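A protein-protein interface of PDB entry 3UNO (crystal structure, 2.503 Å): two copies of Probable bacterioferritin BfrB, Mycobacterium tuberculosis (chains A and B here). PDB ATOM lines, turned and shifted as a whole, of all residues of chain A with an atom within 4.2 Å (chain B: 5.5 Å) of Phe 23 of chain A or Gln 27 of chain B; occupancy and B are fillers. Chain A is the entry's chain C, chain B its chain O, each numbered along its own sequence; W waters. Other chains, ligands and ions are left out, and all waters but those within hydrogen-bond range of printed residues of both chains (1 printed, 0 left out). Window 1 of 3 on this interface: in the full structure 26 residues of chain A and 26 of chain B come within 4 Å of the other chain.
N of Val 78 of chain A lies within hydrogen-bond range of O of Val 78 of chain B. O of Pro 76 of chain A is in hydrogen-bond range of NE2 of Gln 27 of chain B, 3.0 Å away.
Of the 14 printed residues of chain B, 6 touch a printed residue of chain A. Along chain B the printed residues that touch a printed residue of chain A span positions 23 to 81. Of the 14 printed residues of chain A, 6 touch a printed residue of chain B. Among the printed residues, no Asp or Glu carboxylate lies within 4 Å of a Lys or Arg side-chain nitrogen of the other chain.
Among the printed residues, pairs that only touch across the chains: Phe 23 of chain A with Gln 27 of chain B, Gln 27 of chain A with Phe 23 of chain B, Met 60 of chain A with Val 30 of chain B, Ile 75 of chain A with Gln 27 of chain B, Ile 75 of chain A with Val 30 of chain B, Ile 75 of chain A with Ala 31 of chain B and Ile 75 of chain A with Val 81 of chain B.
Of chain B, only Gln 27 comes within 4 Å of Phe 23 of chain A. Gln 27 of chain B touches three residues of chain A. Of the printed residues of chain A, Val 81 of chain B touches Ile 75. Of the printed residues of chain A, Phe 23 of chain B touches Gln 27 (3.8 Å). Of the printed residues of chain A, Ala 31 of chain B touches Ile 75. Of the printed residues of chain B, Pro 76 of chain A touches Gln 27 (3.0 Å). Of the printed residues of chain B, Ile 75 of chain A touches Gln 27 (3.4 Å), Val 30 (3.9 Å), Ala 31 (3.7 Å) and Val 81 (3.4 Å). The nearest residue of chain B that does not touch Phe 23 of chain A is Val 30 of chain B (4.6 Å). The nearest printed residue of chain B that does not touch Met 60 of chain A is Ala 31 of chain B (7.1 Å).
Phe 23 of chain A touches Gln 27 of chain B, and with the chains exchanged Gln 27 of chain A touches Phe 23 of chain B. Val 78 of chain B touches its own counterpart, Val 78 of chain A. Of the 9 pairs that touch across the chains among the printed residues, 3 have their exchanged pair printed and touching as well.
Water W1 lies within hydrogen-bond range of the backbone carbonyl oxygen of Ile 75 of chain A (2.6 Å) and the backbone NH of Val 81 of chain B (3.0 Å).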
ATOM      1  N   ILE A  19      24.298 -18.447 -16.255  1.00  0.00           N
ATOM      2  CA  ILE A  19      23.052 -17.983 -15.607  1.00  0.00           C
ATOM      3  C   ILE A  19      22.208 -19.161 -15.090  1.00  0.00           C
ATOM      4  O   ILE A  19      21.748 -19.156 -13.941  1.00  0.00           O
ATOM      5  CB  ILE A  19      22.227 -17.132 -16.564  1.00  0.00           C
ATOM      6  CG1 ILE A  19      22.961 -15.800 -16.741  1.00  0.00           C
ATOM      7  CG2 ILE A  19      20.840 -16.913 -15.993  1.00  0.00           C
ATOM      8  CD1 ILE A  19      22.505 -15.002 -17.912  1.00  0.00           C
ATOM      9  N   HIS A  20      22.042 -20.165 -15.954  1.00  0.00           N
ATOM     10  CA  HIS A  20      21.390 -21.415 -15.631  1.00  0.00           C
ATOM     11  C   HIS A  20      22.123 -22.107 -14.491  1.00  0.00           C
ATOM     12  O   HIS A  20      21.507 -22.608 -13.561  1.00  0.00           O
ATOM     13  CB  HIS A  20      21.379 -22.347 -16.854  1.00  0.00           C
ATOM     14  CG  HIS A  20      20.793 -23.693 -16.565  1.00  0.00           C
ATOM     15  ND1 HIS A  20      19.431 -23.932 -16.550  1.00  0.00           N
ATOM     16  CD2 HIS A  20      21.387 -24.859 -16.211  1.00  0.00           C
ATOM     17  CE1 HIS A  20      19.214 -25.194 -16.217  1.00  0.00           C
ATOM     18  NE2 HIS A  20      20.384 -25.779 -16.004  1.00  0.00           N
ATOM     19  N   ASN A  21      23.444 -22.206 -14.579  1.00  0.00           N
ATOM     20  CA  ASN A  21      24.207 -22.893 -13.536  1.00  0.00           C
ATOM     21  C   ASN A  21      24.067 -22.163 -12.205  1.00  0.00           C
ATOM     22  O   ASN A  21      23.933 -22.795 -11.152  1.00  0.00           O
ATOM     23  CB  ASN A  21      25.733 -22.972 -13.879  1.00  0.00           C
ATOM     24  CG  ASN A  21      26.055 -23.827 -15.126  1.00  0.00           C
ATOM     25  OD1 ASN A  21      25.312 -24.747 -15.497  1.00  0.00           O
ATOM     26  ND2 ASN A  21      27.185 -23.526 -15.759  1.00  0.00           N
ATOM     27  N   GLU A  22      24.093 -20.827 -12.242  1.00  0.00           N
ATOM     28  CA  GLU A  22      23.932 -20.072 -11.005  1.00  0.00           C
ATOM     29  C   GLU A  22      22.542 -20.230 -10.385  1.00  0.00           C
ATOM     30  O   GLU A  22      22.430 -20.404  -9.166  1.00  0.00           O
ATOM     31  CB  GLU A  22      24.296 -18.573 -11.168  1.00  0.00           C
ATOM     32  CG  GLU A  22      25.768 -18.295 -11.489  1.00  0.00           C
ATOM     33  CD  GLU A  22      26.729 -18.649 -10.366  1.00  0.00           C
ATOM     34  OE1 GLU A  22      26.289 -19.256  -9.366  1.00  0.00           O
ATOM     35  OE2 GLU A  22      27.933 -18.303 -10.493  1.00  0.00           O
ATOM     36  N   PHE A  23      21.486 -20.176 -11.205  1.00  0.00           N
ATOM     37  CA  PHE A  23      20.123 -20.414 -10.672  1.00  0.00           C
ATOM     38  C   PHE A  23      20.006 -21.811 -10.046  1.00  0.00           C
ATOM     39  O   PHE A  23      19.350 -22.004  -9.003  1.00  0.00           O
ATOM     40  CB  PHE A  23      19.039 -20.177 -11.732  1.00  0.00           C
ATOM     41  CG  PHE A  23      18.631 -18.742 -11.854  1.00  0.00           C
ATOM     42  CD1 PHE A  23      18.066 -18.071 -10.761  1.00  0.00           C
ATOM     43  CD2 PHE A  23      18.799 -18.050 -13.042  1.00  0.00           C
ATOM     44  CE1 PHE A  23      17.676 -16.710 -10.847  1.00  0.00           C
ATOM     45  CE2 PHE A  23      18.420 -16.681 -13.145  1.00  0.00           C
ATOM     46  CZ  PHE A  23      17.863 -16.013 -12.033  1.00  0.00           C
ATOM     47  N   THR A  24      20.674 -22.779 -10.662  1.00  0.00           N
ATOM     48  CA  THR A  24      20.602 -24.124 -10.154  1.00  0.00           C
ATOM     49  C   THR A  24      21.399 -24.205  -8.833  1.00  0.00           C
ATOM     50  O   THR A  24      20.931 -24.775  -7.822  1.00  0.00           O
ATOM     51  CB  THR A  24      21.100 -25.108 -11.188  1.00  0.00           C
ATOM     52  OG1 THR A  24      20.124 -25.161 -12.238  1.00  0.00           O
ATOM     53  CG2 THR A  24      21.266 -26.508 -10.559  1.00  0.00           C
ATOM     54  N   ALA A  25      22.620 -23.659  -8.835  1.00  0.00           N
ATOM     55  CA  ALA A  25      23.436 -23.615  -7.605  1.00  0.00           C
ATOM     56  C   ALA A  25      22.589 -22.988  -6.446  1.00  0.00           C
ATOM     57  O   ALA A  25      22.527 -23.520  -5.315  1.00  0.00           O
ATOM     58  CB  ALA A  25      24.719 -22.825  -7.833  1.00  0.00           C
ATOM     59  N   ALA A  26      21.915 -21.872  -6.735  1.00  0.00           N
ATOM     60  CA  ALA A  26      21.132 -21.212  -5.695  1.00  0.00           C
ATOM     61  C   ALA A  26      20.032 -22.164  -5.183  1.00  0.00           C
ATOM     62  O   ALA A  26      19.802 -22.264  -3.971  1.00  0.00           O
ATOM     63  CB  ALA A  26      20.529 -19.851  -6.215  1.00  0.00           C
ATOM     64  N   GLN A  27      19.362 -22.874  -6.098  1.00  0.00           N
ATOM     65  CA  GLN A  27      18.306 -23.776  -5.688  1.00  0.00           C
ATOM     66  C   GLN A  27      18.915 -24.894  -4.807  1.00  0.00           C
ATOM     67  O   GLN A  27      18.290 -25.369  -3.841  1.00  0.00           O
ATOM     68  CB  GLN A  27      17.562 -24.352  -6.929  1.00  0.00           C
ATOM     69  CG  GLN A  27      16.244 -25.003  -6.602  1.00  0.00           C
ATOM     70  CD  GLN A  27      15.206 -23.976  -6.213  1.00  0.00           C
ATOM     71  OE1 GLN A  27      15.546 -22.788  -6.057  1.00  0.00           O
ATOM     72  NE2 GLN A  27      13.914 -24.405  -6.101  1.00  0.00           N
ATOM     73  N   ALA A  59      23.739 -14.749 -10.217  1.00  0.00           N
ATOM     74  CA  ALA A  59      22.938 -14.981 -11.409  1.00  0.00           C
ATOM     75  C   ALA A  59      22.413 -13.677 -11.987  1.00  0.00           C
ATOM     76  O   ALA A  59      22.493 -13.439 -13.194  1.00  0.00           O
ATOM     77  CB  ALA A  59      21.785 -15.913 -11.093  1.00  0.00           C
ATOM     78  N   MET A  60      21.874 -12.832 -11.118  1.00  0.00           N
ATOM     79  CA  MET A  60      21.288 -11.586 -11.559  1.00  0.00           C
ATOM     80  C   MET A  60      22.353 -10.599 -12.046  1.00  0.00           C
ATOM     81  O   MET A  60      22.072  -9.703 -12.864  1.00  0.00           O
ATOM     82  CB  MET A  60      20.406 -10.998 -10.468  1.00  0.00           C
ATOM     83  CG  MET A  60      19.153 -11.869 -10.168  1.00  0.00           C
ATOM     84  SD  MET A  60      18.225 -12.326 -11.648  1.00  0.00           S
ATOM     85  CE  MET A  60      17.220 -10.850 -11.945  1.00  0.00           C
ATOM     86  N   ILE A  75      15.771 -16.058 -18.902  1.00  0.00           N
ATOM     87  CA  ILE A  75      15.690 -16.562 -17.543  1.00  0.00           C
ATOM     88  C   ILE A  75      15.303 -18.017 -17.719  1.00  0.00           C
ATOM     89  O   ILE A  75      14.234 -18.323 -18.271  1.00  0.00           O
ATOM     90  CB  ILE A  75      14.657 -15.781 -16.720  1.00  0.00           C
ATOM     91  CG1 ILE A  75      15.127 -14.320 -16.607  1.00  0.00           C
ATOM     92  CG2 ILE A  75      14.494 -16.397 -15.338  1.00  0.00           C
ATOM     93  CD1 ILE A  75      16.454 -14.163 -15.833  1.00  0.00           C
ATOM     94  N   PRO A  76      16.176 -18.937 -17.274  1.00  0.00           N
ATOM     95  CA  PRO A  76      15.961 -20.350 -17.620  1.00  0.00           C
ATOM     96  C   PRO A  76      15.145 -21.067 -16.546  1.00  0.00           C
ATOM     97  O   PRO A  76      14.802 -20.468 -15.515  1.00  0.00           O
ATOM     98  CB  PRO A  76      17.388 -20.915 -17.610  1.00  0.00           C
ATOM     99  CG  PRO A  76      18.008 -20.152 -16.391  1.00  0.00           C
ATOM    100  CD  PRO A  76      17.341 -18.758 -16.383  1.00  0.00           C
ATOM    101  N   VAL A  78      15.225 -24.534 -13.938  1.00  0.00           N
ATOM    102  CA  VAL A  78      16.244 -24.931 -12.986  1.00  0.00           C
ATOM    103  C   VAL A  78      16.228 -26.468 -12.883  1.00  0.00           C
ATOM    104  O   VAL A  78      15.164 -27.091 -12.711  1.00  0.00           O
ATOM    105  CB  VAL A  78      15.933 -24.320 -11.604  1.00  0.00           C
ATOM    106  CG1 VAL A  78      16.901 -24.885 -10.535  1.00  0.00           C
ATOM    107  CG2 VAL A  78      15.997 -22.793 -11.643  1.00  0.00           C
ATOM    108  N   GLU B  22       4.889 -22.560  -7.087  1.00  0.00           N
ATOM    109  CA  GLU B  22       5.279 -21.234  -6.624  1.00  0.00           C
ATOM    110  C   GLU B  22       6.710 -20.878  -7.053  1.00  0.00           C
ATOM    111  O   GLU B  22       6.982 -19.731  -7.420  1.00  0.00           O
ATOM    112  CB  GLU B  22       5.081 -21.040  -5.098  1.00  0.00           C
ATOM    113  CG  GLU B  22       3.633 -21.153  -4.624  1.00  0.00           C
ATOM    114  CD  GLU B  22       2.740 -19.943  -5.023  1.00  0.00           C
ATOM    115  OE1 GLU B  22       3.181 -19.091  -5.838  1.00  0.00           O
ATOM    116  OE2 GLU B  22       1.589 -19.851  -4.501  1.00  0.00           O
ATOM    117  N   PHE B  23       7.631 -21.845  -7.001  1.00  0.00           N
ATOM    118  CA  PHE B  23       8.992 -21.562  -7.472  1.00  0.00           C
ATOM    119  C   PHE B  23       8.970 -21.245  -8.959  1.00  0.00           C
ATOM    120  O   PHE B  23       9.781 -20.430  -9.454  1.00  0.00           O
ATOM    121  CB  PHE B  23       9.978 -22.709  -7.172  1.00  0.00           C
ATOM    122  CG  PHE B  23      10.604 -22.628  -5.797  1.00  0.00           C
ATOM    123  CD1 PHE B  23      11.381 -21.526  -5.431  1.00  0.00           C
ATOM    124  CD2 PHE B  23      10.391 -23.627  -4.859  1.00  0.00           C
ATOM    125  CE1 PHE B  23      11.950 -21.425  -4.167  1.00  0.00           C
ATOM    126  CE2 PHE B  23      10.963 -23.548  -3.592  1.00  0.00           C
ATOM    127  CZ  PHE B  23      11.750 -22.442  -3.247  1.00  0.00           C
ATOM    128  N   THR B  24       8.019 -21.848  -9.672  1.00  0.00           N
ATOM    129  CA  THR B  24       7.973 -21.645 -11.125  1.00  0.00           C
ATOM    130  C   THR B  24       7.392 -20.281 -11.372  1.00  0.00           C
ATOM    131  O   THR B  24       7.936 -19.505 -12.180  1.00  0.00           O
ATOM    132  CB  THR B  24       7.192 -22.764 -11.845  1.00  0.00           C
ATOM    133  OG1 THR B  24       7.968 -23.978 -11.750  1.00  0.00           O
ATOM    134  CG2 THR B  24       6.954 -22.394 -13.308  1.00  0.00           C
ATOM    135  N   ALA B  25       6.320 -19.976 -10.635  1.00  0.00           N
ATOM    136  CA  ALA B  25       5.699 -18.658 -10.741  1.00  0.00           C
ATOM    137  C   ALA B  25       6.724 -17.556 -10.470  1.00  0.00           C
ATOM    138  O   ALA B  25       6.784 -16.550 -11.198  1.00  0.00           O
ATOM    139  CB  ALA B  25       4.555 -18.549  -9.808  1.00  0.00           C
ATOM    140  N   ALA B  26       7.564 -17.768  -9.459  1.00  0.00           N
ATOM    141  CA  ALA B  26       8.535 -16.735  -9.080  1.00  0.00           C
ATOM    142  C   ALA B  26       9.534 -16.519 -10.228  1.00  0.00           C
ATOM    143  O   ALA B  26       9.936 -15.374 -10.539  1.00  0.00           O
ATOM    144  CB  ALA B  26       9.272 -17.088  -7.739  1.00  0.00           C
ATOM    145  N   GLN B  27       9.919 -17.615 -10.879  1.00  0.00           N
ATOM    146  CA  GLN B  27      10.918 -17.533 -11.942  1.00  0.00           C
ATOM    147  C   GLN B  27      10.258 -16.840 -13.131  1.00  0.00           C
ATOM    148  O   GLN B  27      10.918 -16.161 -13.918  1.00  0.00           O
ATOM    149  CB  GLN B  27      11.378 -18.953 -12.382  1.00  0.00           C
ATOM    150  CG  GLN B  27      12.656 -18.968 -13.240  1.00  0.00           C
ATOM    151  CD  GLN B  27      13.887 -18.603 -12.426  1.00  0.00           C
ATOM    152  OE1 GLN B  27      13.775 -18.171 -11.256  1.00  0.00           O
ATOM    153  NE2 GLN B  27      15.072 -18.779 -13.026  1.00  0.00           N
ATOM    154  N   GLN B  28       8.944 -17.016 -13.288  1.00  0.00           N
ATOM    155  CA  GLN B  28       8.242 -16.386 -14.409  1.00  0.00           C
ATOM    156  C   GLN B  28       8.209 -14.866 -14.234  1.00  0.00           C
ATOM    157  O   GLN B  28       8.369 -14.135 -15.211  1.00  0.00           O
ATOM    158  CB  GLN B  28       6.824 -16.955 -14.575  1.00  0.00           C
ATOM    159  CG  GLN B  28       6.020 -16.314 -15.684  1.00  0.00           C
ATOM    160  CD  GLN B  28       6.639 -16.515 -17.075  1.00  0.00           C
ATOM    161  OE1 GLN B  28       6.402 -17.540 -17.752  1.00  0.00           O
ATOM    162  NE2 GLN B  28       7.453 -15.531 -17.504  1.00  0.00           N
ATOM    163  N   TYR B  29       8.023 -14.400 -12.989  1.00  0.00           N
ATOM    164  CA  TYR B  29       8.090 -12.955 -12.673  1.00  0.00           C
ATOM    165  C   TYR B  29       9.488 -12.370 -12.925  1.00  0.00           C
ATOM    166  O   TYR B  29       9.594 -11.237 -13.372  1.00  0.00           O
ATOM    167  CB  TYR B  29       7.656 -12.672 -11.215  1.00  0.00           C
ATOM    168  CG  TYR B  29       6.140 -12.756 -11.031  1.00  0.00           C
ATOM    169  CD1 TYR B  29       5.290 -12.433 -12.071  1.00  0.00           C
ATOM    170  CD2 TYR B  29       5.569 -13.161  -9.834  1.00  0.00           C
ATOM    171  CE1 TYR B  29       3.912 -12.506 -11.927  1.00  0.00           C
ATOM    172  CE2 TYR B  29       4.188 -13.235  -9.684  1.00  0.00           C
ATOM    173  CZ  TYR B  29       3.371 -12.902 -10.736  1.00  0.00           C
ATOM    174  OH  TYR B  29       1.999 -12.970 -10.604  1.00  0.00           O
ATOM    175  N   VAL B  30      10.549 -13.136 -12.633  1.00  0.00           N
ATOM    176  CA  VAL B  30      11.887 -12.652 -12.893  1.00  0.00           C
ATOM    177  C   VAL B  30      12.022 -12.441 -14.415  1.00  0.00           C
ATOM    178  O   VAL B  30      12.566 -11.411 -14.893  1.00  0.00           O
ATOM    179  CB  VAL B  30      12.980 -13.642 -12.390  1.00  0.00           C
ATOM    180  CG1 VAL B  30      14.360 -13.084 -12.688  1.00  0.00           C
ATOM    181  CG2 VAL B  30      12.858 -13.943 -10.840  1.00  0.00           C
ATOM    182  N   ALA B  31      11.498 -13.402 -15.187  1.00  0.00           N
ATOM    183  CA  ALA B  31      11.550 -13.310 -16.663  1.00  0.00           C
ATOM    184  C   ALA B  31      10.847 -12.030 -17.142  1.00  0.00           C
ATOM    185  O   ALA B  31      11.357 -11.279 -17.982  1.00  0.00           O
ATOM    186  CB  ALA B  31      10.904 -14.545 -17.311  1.00  0.00           C
ATOM    187  N   ILE B  32       9.657 -11.800 -16.620  1.00  0.00           N
ATOM    188  CA  ILE B  32       8.888 -10.620 -16.972  1.00  0.00           C
ATOM    189  C   ILE B  32       9.623  -9.359 -16.533  1.00  0.00           C
ATOM    190  O   ILE B  32       9.600  -8.385 -17.246  1.00  0.00           O
ATOM    191  CB  ILE B  32       7.484 -10.676 -16.341  1.00  0.00           C
ATOM    192  CG1 ILE B  32       6.667 -11.753 -17.061  1.00  0.00           C
ATOM    193  CG2 ILE B  32       6.829  -9.279 -16.419  1.00  0.00           C
ATOM    194  CD1 ILE B  32       5.301 -12.059 -16.450  1.00  0.00           C
ATOM    195  N   VAL B  78      12.734 -26.229 -11.450  1.00  0.00           N
ATOM    196  CA  VAL B  78      11.826 -25.199 -11.941  1.00  0.00           C
ATOM    197  C   VAL B  78      11.671 -25.345 -13.418  1.00  0.00           C
ATOM    198  O   VAL B  78      12.676 -25.453 -14.142  1.00  0.00           O
ATOM    199  CB  VAL B  78      12.371 -23.798 -11.660  1.00  0.00           C
ATOM    200  CG1 VAL B  78      11.475 -22.728 -12.337  1.00  0.00           C
ATOM    201  CG2 VAL B  78      12.568 -23.560 -10.111  1.00  0.00           C
ATOM    202  N   ASP B  79      10.427 -25.370 -13.877  1.00  0.00           N
ATOM    203  CA  ASP B  79      10.178 -25.482 -15.316  1.00  0.00           C
ATOM    204  C   ASP B  79      10.617 -24.234 -16.111  1.00  0.00           C
ATOM    205  O   ASP B  79      10.727 -23.129 -15.566  1.00  0.00           O
ATOM    206  CB  ASP B  79       8.689 -25.775 -15.563  1.00  0.00           C
ATOM    207  CG  ASP B  79       8.294 -27.157 -15.109  1.00  0.00           C
ATOM    208  OD1 ASP B  79       9.189 -28.032 -14.981  1.00  0.00           O
ATOM    209  OD2 ASP B  79       7.091 -27.360 -14.867  1.00  0.00           O
ATOM    210  N   VAL B  81      10.290 -21.032 -18.439  1.00  0.00           N
ATOM    211  CA  VAL B  81       9.279 -19.986 -18.274  1.00  0.00           C
ATOM    212  C   VAL B  81       9.376 -19.119 -19.495  1.00  0.00           C
ATOM    213  O   VAL B  81      10.319 -19.254 -20.284  1.00  0.00           O
ATOM    214  CB  VAL B  81       9.542 -19.109 -17.045  1.00  0.00           C
ATOM    215  CG1 VAL B  81       9.365 -19.905 -15.756  1.00  0.00           C
ATOM    216  CG2 VAL B  81      11.008 -18.516 -17.103  1.00  0.00           C
HETATM  217  O   HOH W   1      13.163 -20.517 -19.213  1.00  0.00           O
